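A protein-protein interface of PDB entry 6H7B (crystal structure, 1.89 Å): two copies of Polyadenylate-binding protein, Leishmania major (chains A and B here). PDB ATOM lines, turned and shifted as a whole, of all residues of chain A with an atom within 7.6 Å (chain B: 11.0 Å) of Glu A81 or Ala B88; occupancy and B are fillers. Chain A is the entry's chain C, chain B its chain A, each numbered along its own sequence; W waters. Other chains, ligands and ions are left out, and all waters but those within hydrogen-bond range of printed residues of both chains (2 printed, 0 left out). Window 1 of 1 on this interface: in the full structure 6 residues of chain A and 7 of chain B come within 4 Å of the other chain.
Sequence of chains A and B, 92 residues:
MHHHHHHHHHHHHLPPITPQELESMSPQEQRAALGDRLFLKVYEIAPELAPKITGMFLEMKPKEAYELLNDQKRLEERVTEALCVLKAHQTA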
ATOM      1  N   ILE A  53      -0.683   6.698  -8.294  1.00  0.00           N
ATOM      2  CA  ILE A  53      -1.818   6.223  -7.511  1.00  0.00           C
ATOM      3  C   ILE A  53      -2.213   4.815  -7.935  1.00  0.00           C
ATOM      4  O   ILE A  53      -2.490   3.952  -7.088  1.00  0.00           O
ATOM      5  CB  ILE A  53      -2.992   7.212  -7.634  1.00  0.00           C
ATOM      6  CG1 ILE A  53      -2.646   8.529  -6.936  1.00  0.00           C
ATOM      7  CG2 ILE A  53      -4.261   6.632  -7.034  1.00  0.00           C
ATOM      8  CD1 ILE A  53      -3.619   9.657  -7.246  1.00  0.00           C
ATOM      9  N   MET A  56       0.074   2.443  -6.364  1.00  0.00           N
ATOM     10  CA  MET A  56      -0.283   2.253  -4.963  1.00  0.00           C
ATOM     11  C   MET A  56      -1.464   1.301  -4.825  1.00  0.00           C
ATOM     12  O   MET A  56      -1.472   0.432  -3.945  1.00  0.00           O
ATOM     13  CB  MET A  56      -0.596   3.607  -4.319  1.00  0.00           C
ATOM     14  CG  MET A  56       0.578   4.582  -4.322  1.00  0.00           C
ATOM     15  SD  MET A  56       0.109   6.263  -3.865  1.00  0.00           S
ATOM     16  CE  MET A  56      -0.285   6.062  -2.124  1.00  0.00           C
ATOM     17  N   PHE A  57      -2.462   1.443  -5.701  1.00  0.00           N
ATOM     18  CA  PHE A  57      -3.627   0.562  -5.671  1.00  0.00           C
ATOM     19  C   PHE A  57      -3.248  -0.884  -5.967  1.00  0.00           C
ATOM     20  O   PHE A  57      -3.773  -1.814  -5.344  1.00  0.00           O
ATOM     21  CB  PHE A  57      -4.676   1.039  -6.677  1.00  0.00           C
ATOM     22  CG  PHE A  57      -5.406   2.292  -6.263  1.00  0.00           C
ATOM     23  CD1 PHE A  57      -5.148   2.904  -5.048  1.00  0.00           C
ATOM     24  CD2 PHE A  57      -6.373   2.840  -7.092  1.00  0.00           C
ATOM     25  CE1 PHE A  57      -5.834   4.055  -4.672  1.00  0.00           C
ATOM     26  CE2 PHE A  57      -7.060   3.987  -6.725  1.00  0.00           C
ATOM     27  CZ  PHE A  57      -6.790   4.594  -5.514  1.00  0.00           C
ATOM     28  N   LYS A  73     -17.842   5.111  -6.013  1.00  0.00           N
ATOM     29  CA  LYS A  73     -17.764   5.976  -4.841  1.00  0.00           C
ATOM     30  C   LYS A  73     -16.572   5.620  -3.963  1.00  0.00           C
ATOM     31  O   LYS A  73     -15.846   6.511  -3.506  1.00  0.00           O
ATOM     32  CB  LYS A  73     -19.069   5.907  -4.048  1.00  0.00           C
ATOM     33  CG  LYS A  73     -20.164   6.794  -4.620  1.00  0.00           C
ATOM     34  CD  LYS A  73     -19.773   8.263  -4.520  1.00  0.00           C
ATOM     35  CE  LYS A  73     -20.457   9.107  -5.585  1.00  0.00           C
ATOM     36  NZ  LYS A  73     -19.927   8.807  -6.946  1.00  0.00           N
ATOM     37  N   ARG A  74     -16.335   4.326  -3.731  1.00  0.00           N
ATOM     38  CA  ARG A  74     -15.188   3.948  -2.916  1.00  0.00           C
ATOM     39  C   ARG A  74     -13.881   4.124  -3.674  1.00  0.00           C
ATOM     40  O   ARG A  74     -12.838   4.363  -3.055  1.00  0.00           O
ATOM     41  CB  ARG A  74     -15.331   2.510  -2.409  1.00  0.00           C
ATOM     42  CG  ARG A  74     -15.321   2.424  -0.885  1.00  0.00           C
ATOM     43  CD  ARG A  74     -15.602   1.025  -0.365  1.00  0.00           C
ATOM     44  NE  ARG A  74     -14.449   0.138  -0.492  1.00  0.00           N
ATOM     45  CZ  ARG A  74     -14.325  -0.797  -1.428  1.00  0.00           C
ATOM     46  NH1 ARG A  74     -15.289  -0.974  -2.322  1.00  0.00           N
ATOM     47  NH2 ARG A  74     -13.241  -1.561  -1.467  1.00  0.00           N
ATOM     48  N   LEU A  75     -13.913   4.030  -5.005  1.00  0.00           N
ATOM     49  CA  LEU A  75     -12.717   4.331  -5.783  1.00  0.00           C
ATOM     50  C   LEU A  75     -12.295   5.782  -5.596  1.00  0.00           C
ATOM     51  O   LEU A  75     -11.108   6.075  -5.403  1.00  0.00           O
ATOM     52  CB  LEU A  75     -12.959   4.038  -7.261  1.00  0.00           C
ATOM     53  CG  LEU A  75     -11.816   4.515  -8.153  1.00  0.00           C
ATOM     54  CD1 LEU A  75     -10.562   3.695  -7.890  1.00  0.00           C
ATOM     55  CD2 LEU A  75     -12.212   4.453  -9.611  1.00  0.00           C
ATOM     56  N   GLU A  76     -13.257   6.705  -5.645  1.00  0.00           N
ATOM     57  CA  GLU A  76     -12.942   8.115  -5.443  1.00  0.00           C
ATOM     58  C   GLU A  76     -12.414   8.370  -4.035  1.00  0.00           C
ATOM     59  O   GLU A  76     -11.484   9.165  -3.850  1.00  0.00           O
ATOM     60  CB  GLU A  76     -14.180   8.965  -5.737  1.00  0.00           C
ATOM     61  CG  GLU A  76     -14.581   8.908  -7.211  1.00  0.00           C
ATOM     62  CD  GLU A  76     -16.002   9.356  -7.473  1.00  0.00           C
ATOM     63  OE1 GLU A  76     -16.360   9.507  -8.661  1.00  0.00           O
ATOM     64  OE2 GLU A  76     -16.762   9.551  -6.500  1.00  0.00           O
ATOM     65  N   GLU A  77     -12.990   7.704  -3.028  1.00  0.00           N
ATOM     66  CA  GLU A  77     -12.467   7.822  -1.669  1.00  0.00           C
ATOM     67  C   GLU A  77     -11.015   7.361  -1.590  1.00  0.00           C
ATOM     68  O   GLU A  77     -10.187   8.006  -0.934  1.00  0.00           O
ATOM     69  CB  GLU A  77     -13.328   7.014  -0.695  1.00  0.00           C
ATOM     70  CG  GLU A  77     -14.510   7.766  -0.120  1.00  0.00           C
ATOM     71  CD  GLU A  77     -15.198   6.997   0.993  1.00  0.00           C
ATOM     72  OE1 GLU A  77     -14.903   5.794   1.156  1.00  0.00           O
ATOM     73  OE2 GLU A  77     -16.029   7.598   1.707  1.00  0.00           O
ATOM     74  N   ARG A  78     -10.685   6.248  -2.253  1.00  0.00           N
ATOM     75  CA  ARG A  78      -9.320   5.729  -2.200  1.00  0.00           C
ATOM     76  C   ARG A  78      -8.333   6.643  -2.911  1.00  0.00           C
ATOM     77  O   ARG A  78      -7.165   6.719  -2.507  1.00  0.00           O
ATOM     78  CB  ARG A  78      -9.255   4.329  -2.809  1.00  0.00           C
ATOM     79  CG  ARG A  78      -9.978   3.271  -2.020  1.00  0.00           C
ATOM     80  CD  ARG A  78      -9.319   3.017  -0.677  1.00  0.00           C
ATOM     81  NE  ARG A  78     -10.052   1.992   0.055  1.00  0.00           N
ATOM     82  CZ  ARG A  78      -9.730   0.703   0.062  1.00  0.00           C
ATOM     83  NH1 ARG A  78      -8.672   0.277  -0.614  1.00  0.00           N
ATOM     84  NH2 ARG A  78     -10.465  -0.157   0.750  1.00  0.00           N
ATOM     85  N   VAL A  79      -8.763   7.321  -3.979  1.00  0.00           N
ATOM     86  CA  VAL A  79      -7.888   8.291  -4.632  1.00  0.00           C
ATOM     87  C   VAL A  79      -7.601   9.458  -3.692  1.00  0.00           C
ATOM     88  O   VAL A  79      -6.453   9.905  -3.569  1.00  0.00           O
ATOM     89  CB  VAL A  79      -8.506   8.770  -5.959  1.00  0.00           C
ATOM     90  CG1 VAL A  79      -7.644   9.868  -6.574  1.00  0.00           C
ATOM     91  CG2 VAL A  79      -8.660   7.598  -6.938  1.00  0.00           C
ATOM     92  N   THR A  80      -8.632   9.961  -3.012  1.00  0.00           N
ATOM     93  CA  THR A  80      -8.428  11.000  -2.006  1.00  0.00           C
ATOM     94  C   THR A  80      -7.476  10.526  -0.915  1.00  0.00           C
ATOM     95  O   THR A  80      -6.581  11.268  -0.490  1.00  0.00           O
ATOM     96  CB  THR A  80      -9.773  11.411  -1.401  1.00  0.00           C
ATOM     97  OG1 THR A  80     -10.591  12.006  -2.414  1.00  0.00           O
ATOM     98  CG2 THR A  80      -9.579  12.402  -0.256  1.00  0.00           C
ATOM     99  N   GLU A  81      -7.655   9.287  -0.454  1.00  0.00           N
ATOM    100  CA  GLU A  81      -6.772   8.726   0.564  1.00  0.00           C
ATOM    101  C   GLU A  81      -5.326   8.696   0.080  1.00  0.00           C
ATOM    102  O   GLU A  81      -4.409   9.107   0.800  1.00  0.00           O
ATOM    103  CB  GLU A  81      -7.250   7.323   0.936  1.00  0.00           C
ATOM    104  CG  GLU A  81      -6.424   6.627   2.024  1.00  0.00           C
ATOM    105  CD  GLU A  81      -6.834   5.176   2.239  1.00  0.00           C
ATOM    106  OE1 GLU A  81      -5.978   4.370   2.669  1.00  0.00           O
ATOM    107  OE2 GLU A  81      -8.010   4.835   1.983  1.00  0.00           O
ATOM    108  N   ALA A  82      -5.108   8.215  -1.147  1.00  0.00           N
ATOM    109  CA  ALA A  82      -3.757   8.131  -1.694  1.00  0.00           C
ATOM    110  C   ALA A  82      -3.133   9.513  -1.847  1.00  0.00           C
ATOM    111  O   ALA A  82      -1.949   9.703  -1.546  1.00  0.00           O
ATOM    112  CB  ALA A  82      -3.782   7.408  -3.041  1.00  0.00           C
ATOM    113  N   LEU A  83      -3.911  10.485  -2.327  1.00  0.00           N
ATOM    114  CA  LEU A  83      -3.415  11.855  -2.414  1.00  0.00           C
ATOM    115  C   LEU A  83      -3.022  12.384  -1.041  1.00  0.00           C
ATOM    116  O   LEU A  83      -2.006  13.075  -0.898  1.00  0.00           O
ATOM    117  CB  LEU A  83      -4.476  12.756  -3.043  1.00  0.00           C
ATOM    118  CG  LEU A  83      -4.732  12.552  -4.545  1.00  0.00           C
ATOM    119  CD1 LEU A  83      -5.891  13.407  -5.021  1.00  0.00           C
ATOM    120  CD2 LEU A  83      -3.472  12.859  -5.338  1.00  0.00           C
ATOM    121  N   CYS A  84      -3.825  12.080  -0.022  1.00  0.00           N
ATOM    122  CA  CYS A  84      -3.490  12.495   1.336  1.00  0.00           C
ATOM    123  C   CYS A  84      -2.174  11.879   1.794  1.00  0.00           C
ATOM    124  O   CYS A  84      -1.341  12.562   2.408  1.00  0.00           O
ATOM    125  CB  CYS A  84      -4.629  12.123   2.283  1.00  0.00           C
ATOM    126  SG  CYS A  84      -4.303  12.442   4.026  1.00  0.00           S
ATOM    127  N   VAL A  85      -1.967  10.590   1.505  1.00  0.00           N
ATOM    128  CA  VAL A  85      -0.721   9.927   1.884  1.00  0.00           C
ATOM    129  C   VAL A  85       0.465  10.547   1.147  1.00  0.00           C
ATOM    130  O   VAL A  85       1.520  10.804   1.744  1.00  0.00           O
ATOM    131  CB  VAL A  85      -0.825   8.411   1.632  1.00  0.00           C
ATOM    132  CG1 VAL A  85       0.524   7.733   1.835  1.00  0.00           C
ATOM    133  CG2 VAL A  85      -1.868   7.794   2.557  1.00  0.00           C
ATOM    134  N   LEU A  86       0.314  10.806  -0.155  1.00  0.00           N
ATOM    135  CA  LEU A  86       1.393  11.434  -0.917  1.00  0.00           C
ATOM    136  C   LEU A  86       1.714  12.828  -0.387  1.00  0.00           C
ATOM    137  O   LEU A  86       2.886  13.209  -0.293  1.00  0.00           O
ATOM    138  CB  LEU A  86       1.022  11.493  -2.402  1.00  0.00           C
ATOM    139  CG  LEU A  86       0.953  10.126  -3.097  1.00  0.00           C
ATOM    140  CD1 LEU A  86       0.275  10.217  -4.454  1.00  0.00           C
ATOM    141  CD2 LEU A  86       2.347   9.525  -3.236  1.00  0.00           C
ATOM    142  N   LYS A  87       0.686  13.605  -0.039  1.00  0.00           N
ATOM    143  CA  LYS A  87       0.918  14.936   0.512  1.00  0.00           C
ATOM    144  C   LYS A  87       1.680  14.860   1.829  1.00  0.00           C
ATOM    145  O   LYS A  87       2.617  15.633   2.059  1.00  0.00           O
ATOM    146  CB  LYS A  87      -0.414  15.665   0.704  1.00  0.00           C
ATOM    147  CG  LYS A  87      -0.279  17.075   1.274  1.00  0.00           C
ATOM    148  CD  LYS A  87      -1.625  17.645   1.673  1.00  0.00           C
ATOM    149  CE  LYS A  87      -1.474  19.053   2.230  1.00  0.00           C
ATOM    150  NZ  LYS A  87      -2.519  19.366   3.243  1.00  0.00           N
ATOM    151  N   LEU B  49      -7.694  12.749  17.996  1.00  0.00           N
ATOM    152  CA  LEU B  49      -8.245  11.586  17.307  1.00  0.00           C
ATOM    153  C   LEU B  49      -7.667  10.266  17.809  1.00  0.00           C
ATOM    154  O   LEU B  49      -7.925   9.222  17.203  1.00  0.00           O
ATOM    155  CB  LEU B  49      -8.028  11.711  15.799  1.00  0.00           C
ATOM    156  CG  LEU B  49      -8.801  12.851  15.131  1.00  0.00           C
ATOM    157  CD1 LEU B  49      -8.465  12.937  13.660  1.00  0.00           C
ATOM    158  CD2 LEU B  49     -10.297  12.671  15.329  1.00  0.00           C
ATOM    159  N   MET B  56      -9.167   1.934  15.292  1.00  0.00           N
ATOM    160  CA  MET B  56      -8.853   1.440  13.953  1.00  0.00           C
ATOM    161  C   MET B  56      -7.695   0.449  13.988  1.00  0.00           C
ATOM    162  O   MET B  56      -7.734  -0.587  13.312  1.00  0.00           O
ATOM    163  CB  MET B  56      -8.541   2.616  13.025  1.00  0.00           C
ATOM    164  CG  MET B  56      -9.731   3.564  12.805  1.00  0.00           C
ATOM    165  SD  MET B  56      -9.324   5.139  12.001  1.00  0.00           S
ATOM    166  CE  MET B  56      -8.908   4.605  10.343  1.00  0.00           C
ATOM    167  N   PHE B  57      -6.662   0.740  14.786  1.00  0.00           N
ATOM    168  CA  PHE B  57      -5.519  -0.165  14.905  1.00  0.00           C
ATOM    169  C   PHE B  57      -5.925  -1.502  15.508  1.00  0.00           C
ATOM    170  O   PHE B  57      -5.414  -2.556  15.108  1.00  0.00           O
ATOM    171  CB  PHE B  57      -4.424   0.470  15.768  1.00  0.00           C
ATOM    172  CG  PHE B  57      -3.695   1.607  15.106  1.00  0.00           C
ATOM    173  CD1 PHE B  57      -3.944   1.948  13.786  1.00  0.00           C
ATOM    174  CD2 PHE B  57      -2.742   2.319  15.809  1.00  0.00           C
ATOM    175  CE1 PHE B  57      -3.259   2.990  13.188  1.00  0.00           C
ATOM    176  CE2 PHE B  57      -2.052   3.364  15.219  1.00  0.00           C
ATOM    177  CZ  PHE B  57      -2.313   3.702  13.911  1.00  0.00           C
ATOM    178  N   GLU B  77       3.807   5.967  10.495  1.00  0.00           N
ATOM    179  CA  GLU B  77       3.231   5.783   9.165  1.00  0.00           C
ATOM    180  C   GLU B  77       1.778   5.331   9.248  1.00  0.00           C
ATOM    181  O   GLU B  77       0.934   5.795   8.471  1.00  0.00           O
ATOM    182  CB  GLU B  77       4.051   4.771   8.364  1.00  0.00           C
ATOM    183  CG  GLU B  77       5.440   5.240   7.989  1.00  0.00           C
ATOM    184  CD  GLU B  77       6.194   4.212   7.167  1.00  0.00           C
ATOM    185  OE1 GLU B  77       5.858   3.011   7.261  1.00  0.00           O
ATOM    186  OE2 GLU B  77       7.119   4.605   6.424  1.00  0.00           O
ATOM    187  N   ARG B  78       1.471   4.419  10.178  1.00  0.00           N
ATOM    188  CA  ARG B  78       0.100   3.932  10.331  1.00  0.00           C
ATOM    189  C   ARG B  78      -0.828   5.005  10.879  1.00  0.00           C
ATOM    190  O   ARG B  78      -2.025   4.995  10.574  1.00  0.00           O
ATOM    191  CB  ARG B  78       0.057   2.707  11.247  1.00  0.00           C
ATOM    192  CG  ARG B  78       0.631   1.431  10.654  1.00  0.00           C
ATOM    193  CD  ARG B  78      -0.196   0.924   9.484  1.00  0.00           C
ATOM    194  NE  ARG B  78       0.286  -0.372   9.006  1.00  0.00           N
ATOM    195  CZ  ARG B  78      -0.075  -0.927   7.853  1.00  0.00           C
ATOM    196  NH1 ARG B  78      -0.920  -0.303   7.045  1.00  0.00           N
ATOM    197  NH2 ARG B  78       0.417  -2.109   7.501  1.00  0.00           N
ATOM    198  N   VAL B  79      -0.318   5.918  11.709  1.00  0.00           N
ATOM    199  CA  VAL B  79      -1.156   7.027  12.155  1.00  0.00           C
ATOM    200  C   VAL B  79      -1.497   7.935  10.977  1.00  0.00           C
ATOM    201  O   VAL B  79      -2.653   8.342  10.803  1.00  0.00           O
ATOM    202  CB  VAL B  79      -0.471   7.801  13.296  1.00  0.00           C
ATOM    203  CG1 VAL B  79      -1.213   9.090  13.571  1.00  0.00           C
ATOM    204  CG2 VAL B  79      -0.417   6.946  14.570  1.00  0.00           C
ATOM    205  N   THR B  80      -0.500   8.256  10.150  1.00  0.00           N
ATOM    206  CA  THR B  80      -0.745   9.041   8.943  1.00  0.00           C
ATOM    207  C   THR B  80      -1.751   8.349   8.032  1.00  0.00           C
ATOM    208  O   THR B  80      -2.672   8.991   7.512  1.00  0.00           O
ATOM    209  CB  THR B  80       0.575   9.288   8.207  1.00  0.00           C
ATOM    210  OG1 THR B  80       1.387  10.186   8.974  1.00  0.00           O
ATOM    211  CG2 THR B  80       0.338   9.886   6.815  1.00  0.00           C
ATOM    212  N   GLU B  81      -1.599   7.036   7.838  1.00  0.00           N
ATOM    213  CA  GLU B  81      -2.552   6.299   7.013  1.00  0.00           C
ATOM    214  C   GLU B  81      -3.961   6.381   7.589  1.00  0.00           C
ATOM    215  O   GLU B  81      -4.934   6.551   6.845  1.00  0.00           O
ATOM    216  CB  GLU B  81      -2.119   4.839   6.874  1.00  0.00           C
ATOM    217  CG  GLU B  81      -0.846   4.628   6.063  1.00  0.00           C
ATOM    218  CD  GLU B  81      -0.334   3.200   6.156  1.00  0.00           C
ATOM    219  OE1 GLU B  81      -1.082   2.333   6.656  1.00  0.00           O
ATOM    220  OE2 GLU B  81       0.816   2.948   5.736  1.00  0.00           O
ATOM    221  N   ALA B  82      -4.090   6.268   8.916  1.00  0.00           N
ATOM    222  CA  ALA B  82      -5.409   6.335   9.538  1.00  0.00           C
ATOM    223  C   ALA B  82      -6.031   7.714   9.371  1.00  0.00           C
ATOM    224  O   ALA B  82      -7.229   7.829   9.081  1.00  0.00           O
ATOM    225  CB  ALA B  82      -5.315   5.971  11.021  1.00  0.00           C
ATOM    226  N   LEU B  83      -5.243   8.771   9.576  1.00  0.00           N
ATOM    227  CA  LEU B  83      -5.756  10.123   9.363  1.00  0.00           C
ATOM    228  C   LEU B  83      -6.218  10.310   7.927  1.00  0.00           C
ATOM    229  O   LEU B  83      -7.247  10.947   7.672  1.00  0.00           O
ATOM    230  CB  LEU B  83      -4.685  11.152   9.711  1.00  0.00           C
ATOM    231  CG  LEU B  83      -4.278  11.208  11.179  1.00  0.00           C
ATOM    232  CD1 LEU B  83      -2.987  11.990  11.315  1.00  0.00           C
ATOM    233  CD2 LEU B  83      -5.394  11.829  12.013  1.00  0.00           C
ATOM    234  N   CYS B  84      -5.473   9.754   6.972  1.00  0.00           N
ATOM    235  CA  CYS B  84      -5.849   9.912   5.573  1.00  0.00           C
ATOM    236  C   CYS B  84      -7.109   9.125   5.243  1.00  0.00           C
ATOM    237  O   CYS B  84      -7.936   9.584   4.444  1.00  0.00           O
ATOM    238  CB  CYS B  84      -4.686   9.506   4.675  1.00  0.00           C
ATOM    239  SG  CYS B  84      -3.374  10.744   4.707  1.00  0.00           S
ATOM    240  N   VAL B  85      -7.280   7.947   5.847  1.00  0.00           N
ATOM    241  CA  VAL B  85      -8.540   7.221   5.705  1.00  0.00           C
ATOM    242  C   VAL B  85      -9.692   8.055   6.250  1.00  0.00           C
ATOM    243  O   VAL B  85     -10.754   8.162   5.621  1.00  0.00           O
ATOM    244  CB  VAL B  85      -8.450   5.847   6.395  1.00  0.00           C
ATOM    245  CG1 VAL B  85      -9.829   5.210   6.511  1.00  0.00           C
ATOM    246  CG2 VAL B  85      -7.515   4.929   5.617  1.00  0.00           C
ATOM    247  N   LEU B  86      -9.487   8.687   7.411  1.00  0.00           N
ATOM    248  CA  LEU B  86     -10.527   9.520   8.010  1.00  0.00           C
ATOM    249  C   LEU B  86     -10.810  10.764   7.171  1.00  0.00           C
ATOM    250  O   LEU B  86     -11.973  11.152   7.005  1.00  0.00           O
ATOM    251  CB  LEU B  86     -10.127   9.914   9.432  1.00  0.00           C
ATOM    252  CG  LEU B  86     -10.081   8.755  10.428  1.00  0.00           C
ATOM    253  CD1 LEU B  86      -9.452   9.187  11.738  1.00  0.00           C
ATOM    254  CD2 LEU B  86     -11.486   8.211  10.660  1.00  0.00           C
ATOM    255  N   LYS B  87      -9.767  11.410   6.642  1.00  0.00           N
ATOM    256  CA  LYS B  87      -9.992  12.579   5.793  1.00  0.00           C
ATOM    257  C   LYS B  87     -10.777  12.205   4.543  1.00  0.00           C
ATOM    258  O   LYS B  87     -11.680  12.941   4.122  1.00  0.00           O
ATOM    259  CB  LYS B  87      -8.662  13.226   5.407  1.00  0.00           C
ATOM    260  CG  LYS B  87      -8.798  14.354   4.377  1.00  0.00           C
ATOM    261  CD  LYS B  87      -7.449  14.794   3.846  1.00  0.00           C
ATOM    262  CE  LYS B  87      -7.598  15.867   2.774  1.00  0.00           C
ATOM    263  NZ  LYS B  87      -6.290  16.157   2.122  1.00  0.00           N
ATOM    264  N   ALA B  88     -10.444  11.064   3.934  1.00  0.00           N
ATOM    265  CA  ALA B  88     -11.149  10.631   2.731  1.00  0.00           C
ATOM    266  C   ALA B  88     -12.588  10.239   3.039  1.00  0.00           C
ATOM    267  O   ALA B  88     -13.459  10.335   2.168  1.00  0.00           O
ATOM    268  CB  ALA B  88     -10.412   9.461   2.077  1.00  0.00           C
ATOM    269  N   HIS B  89     -12.850   9.793   4.267  1.00  0.00           N
ATOM    270  CA  HIS B  89     -14.206   9.434   4.663  1.00  0.00           C
ATOM    271  C   HIS B  89     -15.125  10.650   4.713  1.00  0.00           C
ATOM    272  O   HIS B  89     -16.332  10.519   4.483  1.00  0.00           O
ATOM    273  CB  HIS B  89     -14.172   8.728   6.019  1.00  0.00           C
ATOM    274  CG  HIS B  89     -15.486   8.144   6.425  1.00  0.00           C
ATOM    275  ND1 HIS B  89     -16.120   7.163   5.692  1.00  0.00           N
ATOM    276  CD2 HIS B  89     -16.290   8.404   7.483  1.00  0.00           C
ATOM    277  CE1 HIS B  89     -17.257   6.842   6.283  1.00  0.00           C
ATOM    278  NE2 HIS B  89     -17.383   7.580   7.372  1.00  0.00           N
ATOM    279  N   GLN B  90     -14.583  11.835   5.021  1.00  0.00           N
ATOM    280  CA  GLN B  90     -15.416  13.037   5.058  1.00  0.00           C
ATOM    281  C   GLN B  90     -15.822  13.476   3.661  1.00  0.00           C
ATOM    282  O   GLN B  90     -16.858  14.131   3.492  1.00  0.00           O
ATOM    283  CB  GLN B  90     -14.688  14.184   5.764  1.00  0.00           C
ATOM    284  CG  GLN B  90     -14.062  13.828   7.094  1.00  0.00           C
ATOM    285  CD  GLN B  90     -15.070  13.335   8.114  1.00  0.00           C
ATOM    286  OE1 GLN B  90     -16.251  13.696   8.074  1.00  0.00           O
ATOM    287  NE2 GLN B  90     -14.609  12.502   9.036  1.00  0.00           N
ATOM    288  N   THR B  91     -15.025  13.125   2.657  1.00  0.00           N
ATOM    289  CA  THR B  91     -15.257  13.550   1.283  1.00  0.00           C
ATOM    290  C   THR B  91     -16.244  12.623   0.582  1.00  0.00           C
ATOM    291  O   THR B  91     -16.183  11.404   0.741  1.00  0.00           O
ATOM    292  CB  THR B  91     -13.940  13.583   0.483  1.00  0.00           C
ATOM    293  OG1 THR B  91     -12.898  14.136   1.301  1.00  0.00           O
ATOM    294  CG2 THR B  91     -14.093  14.443  -0.765  1.00  0.00           C
HETATM  295  O   HOH W   1      -6.375  14.141  -0.135  1.00  0.00           O
HETATM  296  O   HOH W   2      -4.069   5.363   4.206  1.00  0.00           O
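Water W2 lies within hydrogen-bond range of OE1 of Glu A81 (2.6 Å) and O of Glu B81 (3.0 Å). Water W1 lies within hydrogen-bond range of the backbone carbonyl oxygen of Thr A80 (2.9 Å), the side-chain amino group of Lys B87 (3.0 Å) and the backbone NH of Cys A84 (3.3 Å).
OG1 of Thr B91 lies within hydrogen-bond range of O of Lys B87, at 3.3 Å. The backbone carbonyl oxygen (O) of Glu A76 is in hydrogen-bond range of the side-chain hydroxyl (OG1) of Thr A80. The guanidinium group (NE) of Arg A78 is in salt-bridge range of the side-chain carboxylate (OE2) of Glu A81, 3.996 Å away.
O of Glu A77 touches CB of Ala B88, 3.4 Å away. Glu A77 touches His B89 (OE2 to CA, 3.9 Å). O of Thr B91 touches OE2 of Glu A77, 3.9 Å away. CG2 of Thr A80 touches CA of Ala B88, 3.8 Å away. CB of Cys B84 touches O of Glu A81 (3.9 Å). Val B85 touches Glu A81 (CG2 to OE1, 3.4 Å). N of Glu A81 touches CB of Ala B88, 3.7 Å away. Lys B87 touches Cys A84 (CD to SG, 3.9 Å).
SG of Cys B84 sits at hydrogen-bond distance from N of Val A85, at 3.5 Å. The side-chain sulfur (SG) of Cys B84 is disulfide-bonded to the side-chain sulfur (SG) of Cys A84, at 2.1 Å.
Of the 18 printed residues of chain B, 6 touch a printed residue of chain A. Printed residues of chain A that touch a printed residue of chain B: Glu A77, Thr A80, Glu A81, Cys A84 and Val A85. Hydrophobic or aromatic side chains of chain A within 4 Å of the printed part of chain B: Val A85. Among the printed residues, no Asp or Glu carboxylate lies within 4 Å of a Lys or Arg side-chain nitrogen of the other chain.
Of chain B, only Cys B84 (3.9 Å), Val B85 (3.4 Å) and Ala B88 (3.7 Å) come within 4 Å of Glu A81. Ala B88 touches three residues of chain A. Of chain B, only Ala B88, His B89 and Thr B91 come within 4 Å of Glu A77. No residue of chain B comes within 4 Å of Arg A78. No residue of chain B comes within 4 Å of Val A79. No residue of chain B comes within 4 Å of Ala A82. Printed residues of chain A within 4 Å of Cys B84: Glu A81, Cys A84 and Val A85. Of the printed residues of chain A, Val B85 touches Glu A81 (3.4 Å). Of the printed residues of chain A, Lys B87 touches Cys A84 (3.9 Å). Of the printed residues of chain A, His B89 touches Glu A77. Gln B90 touches none of the printed residues of chain A. Leu B49 touches none of the printed residues of chain A. The nearest printed residue of chain A that does not touch Cys B84 is Thr A80 (5.4 Å).
Glu A81 touches Val B85, but with the chains exchanged Val A85 does not touch Glu B81 (4.7 Å). Cys A84 touches its own counterpart, Cys B84. Cys A84 touches Lys B87, but with the chains exchanged Lys A87 does not touch Cys B84 (6.9 Å). Val A85 touches Cys B84, but with the chains exchanged Cys A84 does not touch Val B85 (5.7 Å). 13 positions are printed for both chains. Of the 10 pairs that touch across the chains among the printed residues, 1 has its exchanged pair printed and touching as well.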
